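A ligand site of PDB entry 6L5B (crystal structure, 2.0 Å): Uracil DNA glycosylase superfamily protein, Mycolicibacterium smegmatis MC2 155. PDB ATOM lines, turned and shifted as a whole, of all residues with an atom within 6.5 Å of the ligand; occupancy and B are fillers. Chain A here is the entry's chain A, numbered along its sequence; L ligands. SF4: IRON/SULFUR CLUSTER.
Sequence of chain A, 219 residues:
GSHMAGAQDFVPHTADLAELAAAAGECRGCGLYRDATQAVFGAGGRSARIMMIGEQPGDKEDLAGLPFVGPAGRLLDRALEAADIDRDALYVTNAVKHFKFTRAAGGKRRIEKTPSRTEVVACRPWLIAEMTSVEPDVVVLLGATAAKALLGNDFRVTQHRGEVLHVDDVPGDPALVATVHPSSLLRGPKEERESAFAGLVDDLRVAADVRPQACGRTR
SG of Cys 27 sits close to N of Gly 29 (3.2 Å).
NE1 of Trp 126 sits close to SG of Cys 27 (3.4 Å).
The backbone NH (N) of Leu 32 sits close to the side-chain sulfur (SG) of Cys 30, 3.7 Å away.
NE2 of His 98 is in hydrogen-bond range of N of Ala 39 (3.3 Å).
The side-chain sulfur of Cys 123 lies close to the backbone NH of Lys 97 (3.5 Å).
SG of Cys 123 sits close to O of Ala 95, 3.5 Å away.
N of Ala 7 lies within hydrogen-bond range of O of Ala 122.
An iron atom (FE2) of the ligand is bound by the side-chain sulfur of Cys 27, 2.2 Å away.
A sulfur (S1) of the ligand sits close to the backbone NH of Cys 30 (3.5 Å).
The side-chain sulfur (SG) of Cys 30 is bound to an iron atom (FE4) of the ligand (2.2 Å).
The backbone NH (N) of His 98 sits close to a sulfur (S2) of the ligand, 3.8 Å away.
An iron atom (FE3) of the ligand is bound by a ring nitrogen (ND1) of His 98, at 2.2 Å.
An iron atom (FE1) of the ligand is bound by the side-chain sulfur (SG) of Cys 123.
N of Gly 29 sits close to S1 of the ligand (3.7 Å).
A sulfur (S4) of the ligand lies close to the indole nitrogen (NE1) of Trp 126 (3.7 Å).
Merely in contact with the ligand: Tyr 33 (3.9 Å), Val 96 (3.9 Å), Lys 97 (3.97 Å) and Ala 122 (3.9 Å).
Within 4 Å of the ligand: Cys 27, Gly 29, Cys 30, Tyr 33, Val 96, Lys 97, His 98, Ala 122, Cys 123 and Trp 126.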
ATOM      1  N   GLY A   6       7.025  11.162   9.259  1.00  0.00           N
ATOM      2  CA  GLY A   6       5.904  11.183   8.334  1.00  0.00           C
ATOM      3  C   GLY A   6       4.562  11.336   9.013  1.00  0.00           C
ATOM      4  O   GLY A   6       4.370  12.158   9.930  1.00  0.00           O
ATOM      5  N   ALA A   7       3.613  10.523   8.557  1.00  0.00           N
ATOM      6  CA  ALA A   7       2.230  10.637   8.970  1.00  0.00           C
ATOM      7  C   ALA A   7       1.987  10.207  10.408  1.00  0.00           C
ATOM      8  O   ALA A   7       0.878  10.406  10.913  1.00  0.00           O
ATOM      9  CB  ALA A   7       1.352   9.809   8.034  1.00  0.00           C
ATOM     10  N   PHE A  10       0.263  12.314  12.993  1.00  0.00           N
ATOM     11  CA  PHE A  10      -1.096  12.722  12.668  1.00  0.00           C
ATOM     12  C   PHE A  10      -2.117  11.592  12.754  1.00  0.00           C
ATOM     13  O   PHE A  10      -3.315  11.848  12.582  1.00  0.00           O
ATOM     14  CB  PHE A  10      -1.126  13.329  11.261  1.00  0.00           C
ATOM     15  CG  PHE A  10      -0.195  14.496  11.101  1.00  0.00           C
ATOM     16  CD1 PHE A  10      -0.566  15.748  11.539  1.00  0.00           C
ATOM     17  CD2 PHE A  10       1.066  14.313  10.520  1.00  0.00           C
ATOM     18  CE1 PHE A  10       0.294  16.844  11.410  1.00  0.00           C
ATOM     19  CE2 PHE A  10       1.937  15.392  10.384  1.00  0.00           C
ATOM     20  CZ  PHE A  10       1.553  16.663  10.820  1.00  0.00           C
ATOM     21  N   ALA A  24      -7.063  12.187   8.561  1.00  0.00           N
ATOM     22  CA  ALA A  24      -6.128  12.178   7.438  1.00  0.00           C
ATOM     23  C   ALA A  24      -6.187  13.471   6.625  1.00  0.00           C
ATOM     24  O   ALA A  24      -5.200  13.834   5.981  1.00  0.00           O
ATOM     25  CB  ALA A  24      -6.380  10.960   6.549  1.00  0.00           C
ATOM     26  N   CYS A  27      -3.539  15.713   7.925  1.00  0.00           N
ATOM     27  CA  CYS A  27      -2.184  15.197   7.881  1.00  0.00           C
ATOM     28  C   CYS A  27      -1.261  16.147   7.123  1.00  0.00           C
ATOM     29  O   CYS A  27      -1.608  16.652   6.045  1.00  0.00           O
ATOM     30  CB  CYS A  27      -2.143  13.802   7.223  1.00  0.00           C
ATOM     31  SG  CYS A  27      -0.534  13.029   7.302  1.00  0.00           S
ATOM     32  N   ARG A  28      -0.087  16.366   7.683  1.00  0.00           N
ATOM     33  CA  ARG A  28       0.983  17.086   7.007  1.00  0.00           C
ATOM     34  C   ARG A  28       2.244  16.222   6.926  1.00  0.00           C
ATOM     35  O   ARG A  28       3.368  16.734   6.874  1.00  0.00           O
ATOM     36  CB  ARG A  28       1.271  18.409   7.701  1.00  0.00           C
ATOM     37  CG  ARG A  28       0.064  19.342   7.819  1.00  0.00           C
ATOM     38  CD  ARG A  28       0.481  20.751   8.269  1.00  0.00           C
ATOM     39  NE  ARG A  28       1.212  20.718   9.524  1.00  0.00           N
ATOM     40  CZ  ARG A  28       0.640  20.552  10.711  1.00  0.00           C
ATOM     41  NH1 ARG A  28      -0.685  20.399  10.804  1.00  0.00           N
ATOM     42  NH2 ARG A  28       1.381  20.542  11.810  1.00  0.00           N
ATOM     43  N   GLY A  29       2.044  14.901   6.945  1.00  0.00           N
ATOM     44  CA  GLY A  29       3.142  13.930   6.962  1.00  0.00           C
ATOM     45  C   GLY A  29       4.118  14.072   5.815  1.00  0.00           C
ATOM     46  O   GLY A  29       5.265  13.632   5.930  1.00  0.00           O
ATOM     47  N   CYS A  30       3.671  14.632   4.693  1.00  0.00           N
ATOM     48  CA  CYS A  30       4.594  14.988   3.616  1.00  0.00           C
ATOM     49  C   CYS A  30       4.046  16.254   2.963  1.00  0.00           C
ATOM     50  O   CYS A  30       3.150  16.898   3.510  1.00  0.00           O
ATOM     51  CB  CYS A  30       4.792  13.807   2.634  1.00  0.00           C
ATOM     52  SG  CYS A  30       3.439  13.366   1.559  1.00  0.00           S
ATOM     53  N   GLY A  31       4.611  16.632   1.802  1.00  0.00           N
ATOM     54  CA  GLY A  31       4.209  17.881   1.170  1.00  0.00           C
ATOM     55  C   GLY A  31       2.933  17.822   0.349  1.00  0.00           C
ATOM     56  O   GLY A  31       2.385  18.873   0.021  1.00  0.00           O
ATOM     57  N   LEU A  32       2.445  16.608   0.043  1.00  0.00           N
ATOM     58  CA  LEU A  32       1.314  16.413  -0.863  1.00  0.00           C
ATOM     59  C   LEU A  32      -0.005  16.981  -0.356  1.00  0.00           C
ATOM     60  O   LEU A  32      -0.917  17.188  -1.167  1.00  0.00           O
ATOM     61  CB  LEU A  32       1.155  14.908  -1.148  1.00  0.00           C
ATOM     62  CG  LEU A  32       2.356  14.259  -1.849  1.00  0.00           C
ATOM     63  CD1 LEU A  32       2.065  12.817  -2.212  1.00  0.00           C
ATOM     64  CD2 LEU A  32       2.791  15.036  -3.105  1.00  0.00           C
ATOM     65  N   TYR A  33      -0.143  17.226   0.959  1.00  0.00           N
ATOM     66  CA  TYR A  33      -1.406  17.799   1.452  1.00  0.00           C
ATOM     67  C   TYR A  33      -1.645  19.214   0.941  1.00  0.00           C
ATOM     68  O   TYR A  33      -2.793  19.671   0.959  1.00  0.00           O
ATOM     69  CB  TYR A  33      -1.437  17.838   2.994  1.00  0.00           C
ATOM     70  CG  TYR A  33      -0.588  18.942   3.595  1.00  0.00           C
ATOM     71  CD1 TYR A  33      -1.149  20.152   4.027  1.00  0.00           C
ATOM     72  CD2 TYR A  33       0.781  18.784   3.706  1.00  0.00           C
ATOM     73  CE1 TYR A  33      -0.351  21.163   4.562  1.00  0.00           C
ATOM     74  CE2 TYR A  33       1.584  19.787   4.239  1.00  0.00           C
ATOM     75  CZ  TYR A  33       1.019  20.964   4.653  1.00  0.00           C
ATOM     76  OH  TYR A  33       1.865  21.904   5.189  1.00  0.00           O
ATOM     77  N   ARG A  34      -0.603  19.890   0.442  1.00  0.00           N
ATOM     78  CA  ARG A  34      -0.680  21.329   0.205  1.00  0.00           C
ATOM     79  C   ARG A  34      -1.570  21.660  -0.984  1.00  0.00           C
ATOM     80  O   ARG A  34      -2.501  22.469  -0.874  1.00  0.00           O
ATOM     81  CB  ARG A  34       0.707  21.896  -0.027  1.00  0.00           C
ATOM     82  CG  ARG A  34       1.562  21.984   1.218  1.00  0.00           C
ATOM     83  CD  ARG A  34       2.654  23.013   1.002  1.00  0.00           C
ATOM     84  NE  ARG A  34       3.928  22.557   1.549  1.00  0.00           N
ATOM     85  CZ  ARG A  34       4.775  21.777   0.892  1.00  0.00           C
ATOM     86  NH1 ARG A  34       4.488  21.348  -0.332  1.00  0.00           N
ATOM     87  NH2 ARG A  34       5.919  21.413   1.475  1.00  0.00           N
ATOM     88  N   ALA A  39      -7.750  14.723   1.633  1.00  0.00           N
ATOM     89  CA  ALA A  39      -7.268  13.349   1.731  1.00  0.00           C
ATOM     90  C   ALA A  39      -8.245  12.409   1.057  1.00  0.00           C
ATOM     91  O   ALA A  39      -9.474  12.564   1.165  1.00  0.00           O
ATOM     92  CB  ALA A  39      -7.085  12.952   3.199  1.00  0.00           C
ATOM     93  N   ALA A  95      -1.854   3.632  -1.257  1.00  0.00           N
ATOM     94  CA  ALA A  95      -0.649   3.761  -0.441  1.00  0.00           C
ATOM     95  C   ALA A  95      -0.368   5.219  -0.071  1.00  0.00           C
ATOM     96  O   ALA A  95       0.155   5.478   1.017  1.00  0.00           O
ATOM     97  CB  ALA A  95       0.536   3.133  -1.185  1.00  0.00           C
ATOM     98  N   VAL A  96      -0.717   6.165  -0.945  1.00  0.00           N
ATOM     99  CA  VAL A  96      -0.546   7.607  -0.732  1.00  0.00           C
ATOM    100  C   VAL A  96      -1.925   8.253  -0.819  1.00  0.00           C
ATOM    101  O   VAL A  96      -2.701   7.975  -1.740  1.00  0.00           O
ATOM    102  CB  VAL A  96       0.418   8.213  -1.774  1.00  0.00           C
ATOM    103  CG1 VAL A  96       0.410   9.727  -1.699  1.00  0.00           C
ATOM    104  CG2 VAL A  96       1.845   7.691  -1.550  1.00  0.00           C
ATOM    105  N   LYS A  97      -2.230   9.123   0.140  1.00  0.00           N
ATOM    106  CA  LYS A  97      -3.613   9.536   0.355  1.00  0.00           C
ATOM    107  C   LYS A  97      -3.897  10.979  -0.052  1.00  0.00           C
ATOM    108  O   LYS A  97      -5.036  11.435   0.102  1.00  0.00           O
ATOM    109  CB  LYS A  97      -4.007   9.260   1.799  1.00  0.00           C
ATOM    110  CG  LYS A  97      -3.985   7.746   2.072  1.00  0.00           C
ATOM    111  CD  LYS A  97      -4.544   7.397   3.410  1.00  0.00           C
ATOM    112  CE  LYS A  97      -5.061   5.956   3.413  1.00  0.00           C
ATOM    113  NZ  LYS A  97      -4.022   4.913   3.128  1.00  0.00           N
ATOM    114  N   HIS A  98      -2.907  11.690  -0.593  1.00  0.00           N
ATOM    115  CA  HIS A  98      -3.143  12.978  -1.245  1.00  0.00           C
ATOM    116  C   HIS A  98      -2.652  12.912  -2.686  1.00  0.00           C
ATOM    117  O   HIS A  98      -1.578  12.356  -2.968  1.00  0.00           O
ATOM    118  CB  HIS A  98      -2.457  14.144  -0.501  1.00  0.00           C
ATOM    119  CG  HIS A  98      -3.257  14.709   0.640  1.00  0.00           C
ATOM    120  ND1 HIS A  98      -3.013  14.403   1.957  1.00  0.00           N
ATOM    121  CD2 HIS A  98      -4.312  15.567   0.657  1.00  0.00           C
ATOM    122  CE1 HIS A  98      -3.855  15.046   2.735  1.00  0.00           C
ATOM    123  NE2 HIS A  98      -4.656  15.759   1.967  1.00  0.00           N
ATOM    124  N   PHE A  99      -3.457  13.489  -3.586  1.00  0.00           N
ATOM    125  CA  PHE A  99      -3.147  13.552  -5.011  1.00  0.00           C
ATOM    126  C   PHE A  99      -1.835  14.283  -5.266  1.00  0.00           C
ATOM    127  O   PHE A  99      -1.712  15.467  -4.961  1.00  0.00           O
ATOM    128  CB  PHE A  99      -4.299  14.292  -5.716  1.00  0.00           C
ATOM    129  CG  PHE A  99      -4.217  14.308  -7.224  1.00  0.00           C
ATOM    130  CD1 PHE A  99      -3.624  13.272  -7.927  1.00  0.00           C
ATOM    131  CD2 PHE A  99      -4.776  15.368  -7.940  1.00  0.00           C
ATOM    132  CE1 PHE A  99      -3.570  13.286  -9.322  1.00  0.00           C
ATOM    133  CE2 PHE A  99      -4.713  15.387  -9.336  1.00  0.00           C
ATOM    134  CZ  PHE A  99      -4.123  14.340 -10.020  1.00  0.00           C
ATOM    135  N   GLU A 119       7.476   9.847   0.005  1.00  0.00           N
ATOM    136  CA  GLU A 119       6.061  10.081   0.266  1.00  0.00           C
ATOM    137  C   GLU A 119       5.334   8.772   0.592  1.00  0.00           C
ATOM    138  O   GLU A 119       4.435   8.752   1.453  1.00  0.00           O
ATOM    139  CB  GLU A 119       5.445  10.794  -0.933  1.00  0.00           C
ATOM    140  CG  GLU A 119       6.048  12.214  -1.113  1.00  0.00           C
ATOM    141  CD  GLU A 119       5.899  12.730  -2.514  1.00  0.00           C
ATOM    142  OE1 GLU A 119       5.706  11.906  -3.441  1.00  0.00           O
ATOM    143  OE2 GLU A 119       5.966  13.959  -2.694  1.00  0.00           O
ATOM    144  N   ALA A 122       6.323   8.030   4.097  1.00  0.00           N
ATOM    145  CA  ALA A 122       5.697   8.977   5.019  1.00  0.00           C
ATOM    146  C   ALA A 122       4.236   8.662   5.230  1.00  0.00           C
ATOM    147  O   ALA A 122       3.706   8.822   6.334  1.00  0.00           O
ATOM    148  CB  ALA A 122       5.832  10.410   4.492  1.00  0.00           C
ATOM    149  N   CYS A 123       3.537   8.238   4.176  1.00  0.00           N
ATOM    150  CA  CYS A 123       2.114   7.962   4.292  1.00  0.00           C
ATOM    151  C   CYS A 123       1.810   6.568   4.829  1.00  0.00           C
ATOM    152  O   CYS A 123       0.664   6.308   5.231  1.00  0.00           O
ATOM    153  CB  CYS A 123       1.456   8.179   2.919  1.00  0.00           C
ATOM    154  SG  CYS A 123      -0.332   8.420   2.935  1.00  0.00           S
ATOM    155  N   ARG A 124       2.812   5.671   4.880  1.00  0.00           N
ATOM    156  CA  ARG A 124       2.606   4.278   5.297  1.00  0.00           C
ATOM    157  C   ARG A 124       1.944   4.072   6.677  1.00  0.00           C
ATOM    158  O   ARG A 124       1.249   3.059   6.861  1.00  0.00           O
ATOM    159  CB  ARG A 124       3.940   3.526   5.270  1.00  0.00           C
ATOM    160  CG  ARG A 124       3.783   2.013   5.419  1.00  0.00           C
ATOM    161  CD  ARG A 124       5.014   1.272   4.920  1.00  0.00           C
ATOM    162  NE  ARG A 124       6.215   1.733   5.602  1.00  0.00           N
ATOM    163  CZ  ARG A 124       7.453   1.527   5.159  1.00  0.00           C
ATOM    164  NH1 ARG A 124       7.668   0.880   4.016  1.00  0.00           N
ATOM    165  NH2 ARG A 124       8.493   1.980   5.857  1.00  0.00           N
ATOM    166  N   TRP A 126      -0.676   5.446   7.813  1.00  0.00           N
ATOM    167  CA  TRP A 126      -2.116   5.337   7.573  1.00  0.00           C
ATOM    168  C   TRP A 126      -2.472   3.942   7.090  1.00  0.00           C
ATOM    169  O   TRP A 126      -3.514   3.399   7.486  1.00  0.00           O
ATOM    170  CB  TRP A 126      -2.575   6.377   6.549  1.00  0.00           C
ATOM    171  CG  TRP A 126      -2.521   7.793   7.062  1.00  0.00           C
ATOM    172  CD1 TRP A 126      -1.689   8.791   6.648  1.00  0.00           C
ATOM    173  CD2 TRP A 126      -3.330   8.344   8.106  1.00  0.00           C
ATOM    174  NE1 TRP A 126      -1.932   9.938   7.377  1.00  0.00           N
ATOM    175  CE2 TRP A 126      -2.927   9.688   8.276  1.00  0.00           C
ATOM    176  CE3 TRP A 126      -4.346   7.828   8.918  1.00  0.00           C
ATOM    177  CZ2 TRP A 126      -3.507  10.516   9.219  1.00  0.00           C
ATOM    178  CZ3 TRP A 126      -4.931   8.664   9.864  1.00  0.00           C
ATOM    179  CH2 TRP A 126      -4.520   9.991   9.996  1.00  0.00           C
HETATM  180 FE1  SF4 L   1      -0.085  10.625   3.246  1.00  0.00          FE
HETATM  181 FE2  SF4 L   1       0.006  12.780   5.213  1.00  0.00          FE
HETATM  182 FE3  SF4 L   1      -1.238  13.229   2.601  1.00  0.00          FE
HETATM  183 FE4  SF4 L   1       1.655  12.982   2.804  1.00  0.00          FE
HETATM  184  S1  SF4 L   1       0.259  14.399   3.748  1.00  0.00           S
HETATM  185  S2  SF4 L   1       0.181  11.961   1.521  1.00  0.00           S
HETATM  186  S3  SF4 L   1       1.572  11.487   4.409  1.00  0.00           S
HETATM  187  S4  SF4 L   1      -1.678  11.796   4.206  1.00  0.00           S
